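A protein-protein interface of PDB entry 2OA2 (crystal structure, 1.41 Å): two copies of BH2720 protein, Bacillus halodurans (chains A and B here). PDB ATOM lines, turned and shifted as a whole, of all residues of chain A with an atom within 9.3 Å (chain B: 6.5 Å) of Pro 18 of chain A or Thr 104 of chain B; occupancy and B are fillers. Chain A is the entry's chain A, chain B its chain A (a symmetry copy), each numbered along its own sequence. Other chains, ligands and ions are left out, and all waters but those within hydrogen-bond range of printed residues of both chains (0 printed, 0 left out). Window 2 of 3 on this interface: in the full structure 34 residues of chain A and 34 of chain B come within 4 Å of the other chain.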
ATOM      1  N   HIS A  14     -34.074  33.812   9.216  1.00  0.00           N
ATOM      2  CA  HIS A  14     -33.893  33.189  10.521  1.00  0.00           C
ATOM      3  C   HIS A  14     -32.539  32.519  10.719  1.00  0.00           C
ATOM      4  O   HIS A  14     -32.300  31.860  11.742  1.00  0.00           O
ATOM      5  CB  HIS A  14     -35.005  32.171  10.800  1.00  0.00           C
ATOM      6  CG  HIS A  14     -36.324  32.800  11.098  1.00  0.00           C
ATOM      7  ND1 HIS A  14     -37.087  33.428  10.133  1.00  0.00           N
ATOM      8  CD2 HIS A  14     -37.024  32.877  12.246  1.00  0.00           C
ATOM      9  CE1 HIS A  14     -38.202  33.871  10.687  1.00  0.00           C
ATOM     10  NE2 HIS A  14     -38.178  33.566  11.969  1.00  0.00           N
ATOM     11  N   GLY A  15     -31.655  32.643   9.738  1.00  0.00           N
ATOM     12  CA  GLY A  15     -30.355  32.054   9.895  1.00  0.00           C
ATOM     13  C   GLY A  15     -29.522  32.775  10.951  1.00  0.00           C
ATOM     14  O   GLY A  15     -29.647  33.992  11.109  1.00  0.00           O
ATOM     15  N   PRO A  16     -28.642  32.034  11.660  1.00  0.00           N
ATOM     16  CA  PRO A  16     -28.331  30.598  11.615  1.00  0.00           C
ATOM     17  C   PRO A  16     -29.020  29.801  12.723  1.00  0.00           C
ATOM     18  O   PRO A  16     -28.409  28.896  13.248  1.00  0.00           O
ATOM     19  CB  PRO A  16     -26.836  30.594  11.820  1.00  0.00           C
ATOM     20  CG  PRO A  16     -26.644  31.661  12.890  1.00  0.00           C
ATOM     21  CD  PRO A  16     -27.687  32.748  12.542  1.00  0.00           C
ATOM     22  N   ARG A  17     -30.274  30.119  13.028  1.00  0.00           N
ATOM     23  CA  ARG A  17     -30.981  29.462  14.133  1.00  0.00           C
ATOM     24  C   ARG A  17     -31.439  28.056  13.757  1.00  0.00           C
ATOM     25  O   ARG A  17     -31.870  27.819  12.638  1.00  0.00           O
ATOM     26  CB  ARG A  17     -32.277  30.215  14.494  1.00  0.00           C
ATOM     27  CG  ARG A  17     -32.113  31.615  15.046  1.00  0.00           C
ATOM     28  CD  ARG A  17     -31.752  31.662  16.524  1.00  0.00           C
ATOM     29  NE  ARG A  17     -30.437  31.118  16.771  1.00  0.00           N
ATOM     30  CZ  ARG A  17     -29.287  31.734  16.466  1.00  0.00           C
ATOM     31  NH1 ARG A  17     -29.284  32.928  15.905  1.00  0.00           N
ATOM     32  NH2 ARG A  17     -28.155  31.134  16.726  1.00  0.00           N
ATOM     33  N   PRO A  18     -31.435  27.149  14.723  1.00  0.00           N
ATOM     34  CA  PRO A  18     -32.299  25.947  14.578  1.00  0.00           C
ATOM     35  C   PRO A  18     -33.732  26.438  14.290  1.00  0.00           C
ATOM     36  O   PRO A  18     -34.243  27.352  14.956  1.00  0.00           O
ATOM     37  CB  PRO A  18     -32.220  25.280  15.950  1.00  0.00           C
ATOM     38  CG  PRO A  18     -30.925  25.769  16.537  1.00  0.00           C
ATOM     39  CD  PRO A  18     -30.750  27.193  16.026  1.00  0.00           C
ATOM     40  N   PHE A  19     -34.348  25.884  13.234  1.00  0.00           N
ATOM     41  CA  PHE A  19     -35.552  26.473  12.679  1.00  0.00           C
ATOM     42  C   PHE A  19     -36.409  25.414  12.003  1.00  0.00           C
ATOM     43  O   PHE A  19     -35.903  24.590  11.250  1.00  0.00           O
ATOM     44  CB  PHE A  19     -35.119  27.560  11.669  1.00  0.00           C
ATOM     45  CG  PHE A  19     -36.222  28.305  10.975  1.00  0.00           C
ATOM     46  CD1 PHE A  19     -37.209  28.976  11.649  1.00  0.00           C
ATOM     47  CD2 PHE A  19     -36.160  28.453   9.600  1.00  0.00           C
ATOM     48  CE1 PHE A  19     -38.185  29.725  10.972  1.00  0.00           C
ATOM     49  CE2 PHE A  19     -37.110  29.214   8.924  1.00  0.00           C
ATOM     50  CZ  PHE A  19     -38.096  29.844   9.607  1.00  0.00           C
ATOM     51  N   VAL A  20     -37.709  25.472  12.260  1.00  0.00           N
ATOM     52  CA  VAL A  20     -38.709  24.654  11.590  1.00  0.00           C
ATOM     53  C   VAL A  20     -39.741  25.621  10.980  1.00  0.00           C
ATOM     54  O   VAL A  20     -40.163  26.585  11.628  1.00  0.00           O
ATOM     55  CB  VAL A  20     -39.382  23.659  12.602  1.00  0.00           C
ATOM     56  CG1 VAL A  20     -40.613  23.050  12.051  1.00  0.00           C
ATOM     57  CG2 VAL A  20     -38.392  22.613  13.033  1.00  0.00           C
ATOM     58  N   VAL A  21     -40.126  25.329   9.753  1.00  0.00           N
ATOM     59  CA  VAL A  21     -41.019  26.217   8.985  1.00  0.00           C
ATOM     60  C   VAL A  21     -41.877  25.394   8.036  1.00  0.00           C
ATOM     61  O   VAL A  21     -41.416  24.362   7.527  1.00  0.00           O
ATOM     62  CB  VAL A  21     -40.157  27.277   8.230  1.00  0.00           C
ATOM     63  CG1 VAL A  21     -39.247  26.658   7.215  1.00  0.00           C
ATOM     64  CG2 VAL A  21     -41.077  28.372   7.629  1.00  0.00           C
ATOM     65  N   TRP A  38     -33.342  31.714   5.247  1.00  0.00           N
ATOM     66  CA  TRP A  38     -32.392  31.209   6.214  1.00  0.00           C
ATOM     67  C   TRP A  38     -31.000  31.192   5.635  1.00  0.00           C
ATOM     68  O   TRP A  38     -30.722  30.398   4.745  1.00  0.00           O
ATOM     69  CB  TRP A  38     -32.793  29.781   6.654  1.00  0.00           C
ATOM     70  CG  TRP A  38     -32.108  29.262   7.863  1.00  0.00           C
ATOM     71  CD1 TRP A  38     -32.566  29.363   9.142  1.00  0.00           C
ATOM     72  CD2 TRP A  38     -30.825  28.576   7.948  1.00  0.00           C
ATOM     73  NE1 TRP A  38     -31.693  28.726  10.011  1.00  0.00           N
ATOM     74  CE2 TRP A  38     -30.626  28.238   9.303  1.00  0.00           C
ATOM     75  CE3 TRP A  38     -29.855  28.170   7.015  1.00  0.00           C
ATOM     76  CZ2 TRP A  38     -29.511  27.569   9.744  1.00  0.00           C
ATOM     77  CZ3 TRP A  38     -28.754  27.491   7.453  1.00  0.00           C
ATOM     78  CH2 TRP A  38     -28.576  27.198   8.806  1.00  0.00           C
ATOM     79  N   THR A  39     -30.135  31.998   6.221  1.00  0.00           N
ATOM     80  CA  THR A  39     -28.731  32.101   5.820  1.00  0.00           C
ATOM     81  C   THR A  39     -27.864  31.588   6.973  1.00  0.00           C
ATOM     82  O   THR A  39     -27.737  32.218   8.030  1.00  0.00           O
ATOM     83  CB  THR A  39     -28.352  33.537   5.425  1.00  0.00           C
ATOM     84  OG1 THR A  39     -29.255  33.984   4.420  1.00  0.00           O
ATOM     85  CG2 THR A  39     -26.922  33.562   4.931  1.00  0.00           C
ATOM     86  N   GLY A  40     -27.213  30.466   6.724  1.00  0.00           N
ATOM     87  CA  GLY A  40     -26.287  29.852   7.629  1.00  0.00           C
ATOM     88  C   GLY A  40     -24.857  30.085   7.194  1.00  0.00           C
ATOM     89  O   GLY A  40     -24.558  30.857   6.256  1.00  0.00           O
ATOM     90  N   GLU B  59     -27.007  13.275  16.528  1.00  0.00           N
ATOM     91  CA  GLU B  59     -25.749  13.599  15.858  1.00  0.00           C
ATOM     92  C   GLU B  59     -25.455  15.077  15.947  1.00  0.00           C
ATOM     93  O   GLU B  59     -26.279  15.862  16.397  1.00  0.00           O
ATOM     94  CB  GLU B  59     -25.810  13.205  14.400  1.00  0.00           C
ATOM     95  CG  GLU B  59     -24.491  13.134  13.643  1.00  0.00           C
ATOM     96  CD  GLU B  59     -23.359  12.422  14.404  1.00  0.00           C
ATOM     97  OE1 GLU B  59     -22.693  13.084  15.210  1.00  0.00           O
ATOM     98  OE2 GLU B  59     -23.196  11.203  14.222  1.00  0.00           O
ATOM     99  N   ILE B  60     -24.209  15.415  15.596  1.00  0.00           N
ATOM    100  CA  ILE B  60     -23.713  16.784  15.515  1.00  0.00           C
ATOM    101  C   ILE B  60     -22.747  16.784  14.321  1.00  0.00           C
ATOM    102  O   ILE B  60     -21.963  15.858  14.137  1.00  0.00           O
ATOM    103  CB  ILE B  60     -23.096  17.285  16.835  1.00  0.00           C
ATOM    104  CG1 ILE B  60     -22.618  18.733  16.678  1.00  0.00           C
ATOM    105  CG2 ILE B  60     -21.930  16.348  17.322  1.00  0.00           C
ATOM    106  CD1 ILE B  60     -22.241  19.395  17.985  1.00  0.00           C
ATOM    107  N   HIS B  61     -22.859  17.807  13.470  1.00  0.00           N
ATOM    108  CA  HIS B  61     -21.989  18.020  12.316  1.00  0.00           C
ATOM    109  C   HIS B  61     -21.404  19.419  12.398  1.00  0.00           C
ATOM    110  O   HIS B  61     -21.938  20.363  11.863  1.00  0.00           O
ATOM    111  CB  HIS B  61     -22.774  17.825  11.019  1.00  0.00           C
ATOM    112  CG  HIS B  61     -23.148  16.382  10.799  1.00  0.00           C
ATOM    113  ND1 HIS B  61     -24.447  15.932  10.714  1.00  0.00           N
ATOM    114  CD2 HIS B  61     -22.364  15.280  10.768  1.00  0.00           C
ATOM    115  CE1 HIS B  61     -24.438  14.615  10.564  1.00  0.00           C
ATOM    116  NE2 HIS B  61     -23.190  14.197  10.599  1.00  0.00           N
ATOM    117  N   PRO B  62     -20.198  19.555  13.008  1.00  0.00           N
ATOM    118  CA  PRO B  62     -19.639  20.885  13.139  1.00  0.00           C
ATOM    119  C   PRO B  62     -19.214  21.582  11.856  1.00  0.00           C
ATOM    120  O   PRO B  62     -19.003  22.798  11.893  1.00  0.00           O
ATOM    121  CB  PRO B  62     -18.421  20.667  14.073  1.00  0.00           C
ATOM    122  CG  PRO B  62     -18.118  19.268  13.989  1.00  0.00           C
ATOM    123  CD  PRO B  62     -19.355  18.520  13.619  1.00  0.00           C
ATOM    124  N   GLN B  78     -35.520  17.460  17.666  1.00  0.00           N
ATOM    125  CA  GLN B  78     -34.901  17.819  18.958  1.00  0.00           C
ATOM    126  C   GLN B  78     -33.547  18.367  18.668  1.00  0.00           C
ATOM    127  O   GLN B  78     -32.753  17.739  17.938  1.00  0.00           O
ATOM    128  CB  GLN B  78     -34.779  16.583  19.848  1.00  0.00           C
ATOM    129  CG  GLN B  78     -36.084  15.877  20.036  1.00  0.00           C
ATOM    130  CD  GLN B  78     -35.980  14.568  20.782  1.00  0.00           C
ATOM    131  OE1 GLN B  78     -35.185  13.678  20.426  1.00  0.00           O
ATOM    132  NE2 GLN B  78     -36.793  14.441  21.815  1.00  0.00           N
ATOM    133  N   MET B  79     -33.283  19.596  19.172  1.00  0.00           N
ATOM    134  CA  MET B  79     -32.031  20.256  18.912  1.00  0.00           C
ATOM    135  C   MET B  79     -31.510  21.016  20.113  1.00  0.00           C
ATOM    136  O   MET B  79     -32.281  21.470  20.939  1.00  0.00           O
ATOM    137  CB  MET B  79     -32.148  21.235  17.719  1.00  0.00           C
ATOM    138  CG  MET B  79     -32.374  20.554  16.349  1.00  0.00           C
ATOM    139  SD  MET B  79     -32.150  21.648  14.805  1.00  0.00           S
ATOM    140  CE  MET B  79     -33.819  22.240  14.565  1.00  0.00           C
ATOM    141  N   GLY B  80     -30.214  21.082  20.168  1.00  0.00           N
ATOM    142  CA  GLY B  80     -29.588  21.876  21.206  1.00  0.00           C
ATOM    143  C   GLY B  80     -28.162  22.105  20.927  1.00  0.00           C
ATOM    144  O   GLY B  80     -27.488  21.404  20.182  1.00  0.00           O
ATOM    145  N   HIS B  81     -27.725  23.078  21.719  1.00  0.00           N
ATOM    146  CA  HIS B  81     -26.377  23.505  21.884  1.00  0.00           C
ATOM    147  C   HIS B  81     -25.485  22.385  22.481  1.00  0.00           C
ATOM    148  O   HIS B  81     -24.366  22.097  22.053  1.00  0.00           O
ATOM    149  CB  HIS B  81     -26.513  24.674  22.877  1.00  0.00           C
ATOM    150  CG  HIS B  81     -25.370  25.602  22.894  1.00  0.00           C
ATOM    151  ND1 HIS B  81     -24.991  26.262  24.047  1.00  0.00           N
ATOM    152  CD2 HIS B  81     -24.531  26.017  21.923  1.00  0.00           C
ATOM    153  CE1 HIS B  81     -23.955  27.034  23.782  1.00  0.00           C
ATOM    154  NE2 HIS B  81     -23.652  26.903  22.504  1.00  0.00           N
ATOM    155  N   PHE B  88     -34.756  22.640  22.128  1.00  0.00           N
ATOM    156  CA  PHE B  88     -35.601  22.917  20.944  1.00  0.00           C
ATOM    157  C   PHE B  88     -36.302  21.609  20.631  1.00  0.00           C
ATOM    158  O   PHE B  88     -35.637  20.621  20.341  1.00  0.00           O
ATOM    159  CB  PHE B  88     -34.736  23.353  19.782  1.00  0.00           C
ATOM    160  CG  PHE B  88     -35.507  23.707  18.522  1.00  0.00           C
ATOM    161  CD1 PHE B  88     -35.991  22.713  17.706  1.00  0.00           C
ATOM    162  CD2 PHE B  88     -35.736  25.041  18.173  1.00  0.00           C
ATOM    163  CE1 PHE B  88     -36.692  23.079  16.507  1.00  0.00           C
ATOM    164  CE2 PHE B  88     -36.432  25.387  17.029  1.00  0.00           C
ATOM    165  CZ  PHE B  88     -36.921  24.412  16.208  1.00  0.00           C
ATOM    166  N   LEU B  99     -34.137  23.307   9.532  1.00  0.00           N
ATOM    167  CA  LEU B  99     -32.794  23.833   9.312  1.00  0.00           C
ATOM    168  C   LEU B  99     -31.940  23.498  10.534  1.00  0.00           C
ATOM    169  O   LEU B  99     -32.306  23.808  11.702  1.00  0.00           O
ATOM    170  CB  LEU B  99     -32.804  25.323   9.050  1.00  0.00           C
ATOM    171  CG  LEU B  99     -33.128  25.789   7.647  1.00  0.00           C
ATOM    172  CD1 LEU B  99     -32.073  25.289   6.694  1.00  0.00           C
ATOM    173  CD2 LEU B  99     -34.534  25.364   7.206  1.00  0.00           C
ATOM    174  N   ILE B 100     -30.806  22.838  10.274  1.00  0.00           N
ATOM    175  CA  ILE B 100     -29.927  22.308  11.337  1.00  0.00           C
ATOM    176  C   ILE B 100     -28.556  22.931  11.115  1.00  0.00           C
ATOM    177  O   ILE B 100     -27.777  22.468  10.266  1.00  0.00           O
ATOM    178  CB  ILE B 100     -29.844  20.792  11.307  1.00  0.00           C
ATOM    179  CG1 ILE B 100     -31.234  20.137  11.284  1.00  0.00           C
ATOM    180  CG2 ILE B 100     -29.035  20.335  12.502  1.00  0.00           C
ATOM    181  CD1 ILE B 100     -31.254  18.623  11.253  1.00  0.00           C
ATOM    182  N   PRO B 101     -28.286  24.028  11.806  1.00  0.00           N
ATOM    183  CA  PRO B 101     -26.993  24.694  11.561  1.00  0.00           C
ATOM    184  C   PRO B 101     -25.848  23.876  12.113  1.00  0.00           C
ATOM    185  O   PRO B 101     -25.960  23.222  13.160  1.00  0.00           O
ATOM    186  CB  PRO B 101     -27.155  26.056  12.268  1.00  0.00           C
ATOM    187  CG  PRO B 101     -28.106  25.722  13.406  1.00  0.00           C
ATOM    188  CD  PRO B 101     -29.077  24.741  12.841  1.00  0.00           C
ATOM    189  N   ALA B 102     -24.698  23.996  11.490  1.00  0.00           N
ATOM    190  CA  ALA B 102     -23.476  23.350  11.960  1.00  0.00           C
ATOM    191  C   ALA B 102     -23.281  23.618  13.449  1.00  0.00           C
ATOM    192  O   ALA B 102     -23.390  24.750  13.908  1.00  0.00           O
ATOM    193  CB  ALA B 102     -22.286  23.891  11.175  1.00  0.00           C
ATOM    194  N   GLY B 103     -22.887  22.576  14.179  1.00  0.00           N
ATOM    195  CA  GLY B 103     -22.651  22.668  15.600  1.00  0.00           C
ATOM    196  C   GLY B 103     -23.817  22.500  16.544  1.00  0.00           C
ATOM    197  O   GLY B 103     -23.664  22.586  17.756  1.00  0.00           O
ATOM    198  N   THR B 104     -25.000  22.238  15.987  1.00  0.00           N
ATOM    199  CA  THR B 104     -26.199  21.973  16.759  1.00  0.00           C
ATOM    200  C   THR B 104     -26.418  20.431  16.818  1.00  0.00           C
ATOM    201  O   THR B 104     -26.378  19.724  15.793  1.00  0.00           O
ATOM    202  CB  THR B 104     -27.413  22.770  16.165  1.00  0.00           C
ATOM    203  OG1 THR B 104     -27.307  24.184  16.487  1.00  0.00           O
ATOM    204  CG2 THR B 104     -28.702  22.316  16.818  1.00  0.00           C
ATOM    205  N   TRP B 105     -26.548  19.891  18.036  1.00  0.00           N
ATOM    206  CA  TRP B 105     -26.888  18.496  18.243  1.00  0.00           C
ATOM    207  C   TRP B 105     -28.358  18.343  17.803  1.00  0.00           C
ATOM    208  O   TRP B 105     -29.185  19.220  18.081  1.00  0.00           O
ATOM    209  CB  TRP B 105     -26.791  18.136  19.720  1.00  0.00           C
ATOM    210  CG  TRP B 105     -25.397  18.056  20.222  1.00  0.00           C
ATOM    211  CD1 TRP B 105     -24.650  19.078  20.751  1.00  0.00           C
ATOM    212  CD2 TRP B 105     -24.570  16.900  20.225  1.00  0.00           C
ATOM    213  NE1 TRP B 105     -23.408  18.611  21.095  1.00  0.00           N
ATOM    214  CE2 TRP B 105     -23.332  17.273  20.814  1.00  0.00           C
ATOM    215  CE3 TRP B 105     -24.756  15.568  19.839  1.00  0.00           C
ATOM    216  CZ2 TRP B 105     -22.285  16.372  20.980  1.00  0.00           C
ATOM    217  CZ3 TRP B 105     -23.707  14.672  20.020  1.00  0.00           C
ATOM    218  CH2 TRP B 105     -22.492  15.078  20.590  1.00  0.00           C
ATOM    219  N   HIS B 106     -28.673  17.245  17.108  1.00  0.00           N
ATOM    220  CA  HIS B 106     -30.026  17.090  16.580  1.00  0.00           C
ATOM    221  C   HIS B 106     -30.437  15.620  16.481  1.00  0.00           C
ATOM    222  O   HIS B 106     -29.620  14.724  16.282  1.00  0.00           O
ATOM    223  CB  HIS B 106     -30.083  17.741  15.207  1.00  0.00           C
ATOM    224  CG  HIS B 106     -29.043  17.210  14.267  1.00  0.00           C
ATOM    225  ND1 HIS B 106     -27.731  17.639  14.293  1.00  0.00           N
ATOM    226  CD2 HIS B 106     -29.107  16.243  13.327  1.00  0.00           C
ATOM    227  CE1 HIS B 106     -27.045  16.994  13.364  1.00  0.00           C
ATOM    228  NE2 HIS B 106     -27.854  16.138  12.766  1.00  0.00           N
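No position is printed for both chains.
Of the 11 pairs that touch across the chains among the printed residues, none has its exchanged pair printed and touching as well.
The backbone NH (N) of Leu 99 of chain B is in hydrogen-bond range of the backbone carbonyl oxygen (O) of Phe 19 of chain A (2.8 Å).
Printed residues of chain B that touch a printed residue of chain A: Met 79, Phe 88, Leu 99, Pro 101 and Thr 104.
Hydrophobic or aromatic side chains of chain B within 4 Å of the printed part of chain A: Met 79, Phe 88, Leu 99 and Pro 101.
Among the printed residues, 11 pairs touch across the chains.
Among the printed residues, no Asp or Glu carboxylate lies within 4 Å of a Lys or Arg side-chain nitrogen of the other chain.
Pro 16 of chain A touches Pro 101 of chain B.
Pro 18 of chain A touches Met 79 of chain B (CB to CE, 3.7 Å).
Phe 88 of chain B touches Pro 18 of chain A (CE2 to O, 3.6 Å).
CA of Pro 18 of chain A touches O of Leu 99 of chain B, at 3.6 Å.
CD of Pro 101 of chain B touches CA of Pro 18 of chain A, 3.9 Å away.
CG of Pro 18 of chain A touches OG1 of Thr 104 of chain B (3.95 Å).
N of Phe 19 of chain A touches CE of Met 79 of chain B, 3.9 Å away.
CG2 of Val 20 of chain A touches CE1 of Phe 88 of chain B, at 3.9 Å.
Leu 99 of chain B touches Trp 38 of chain A.
Pro 101 of chain B touches Trp 38 of chain A (CB to CZ2, 3.8 Å).
Of the printed residues of chain B, Pro 16 of chain A touches Pro 101 (3.2 Å).
Of chain B, only Met 79 (3.7 Å), Phe 88 (3.6 Å), Leu 99 (3.6 Å), Pro 101 (3.9 Å) and Thr 104 (3.95 Å) come within 4 Å of Pro 18 of chain A.
Printed residues of chain B within 4 Å of Phe 19 of chain A: Met 79 (3.9 Å) and Leu 99 (2.8 Å).
Of the printed residues of chain B, Trp 38 of chain A touches Leu 99 and Pro 101.
Printed residues of chain A within 4 Å of Met 79 of chain B: Pro 18 and Phe 19.
No residue of chain A comes within 4 Å of Gly 103 of chain B.
Thr 104 of chain B touches just one residue of chain A: Pro 18 (3.95 Å).
The nearest residue of chain B that does not touch Pro 18 of chain A is Ile 100 of chain B (5.4 Å).
The nearest residue of chain A that does not touch Thr 104 of chain B is Pro 16 of chain A (5.8 Å).
ND1 of His 106 of chain B sits at hydrogen-bond distance from O of Thr 104 of chain B (2.9 Å).
The indole nitrogen of Trp 38 of chain A sits at hydrogen-bond distance from the backbone carbonyl oxygen of Arg 17 of chain A (2.8 Å).
The backbone NH (N) of Met 79 of chain B is in hydrogen-bond range of the backbone carbonyl oxygen (O) of Phe 88 of chain B (2.8 Å).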
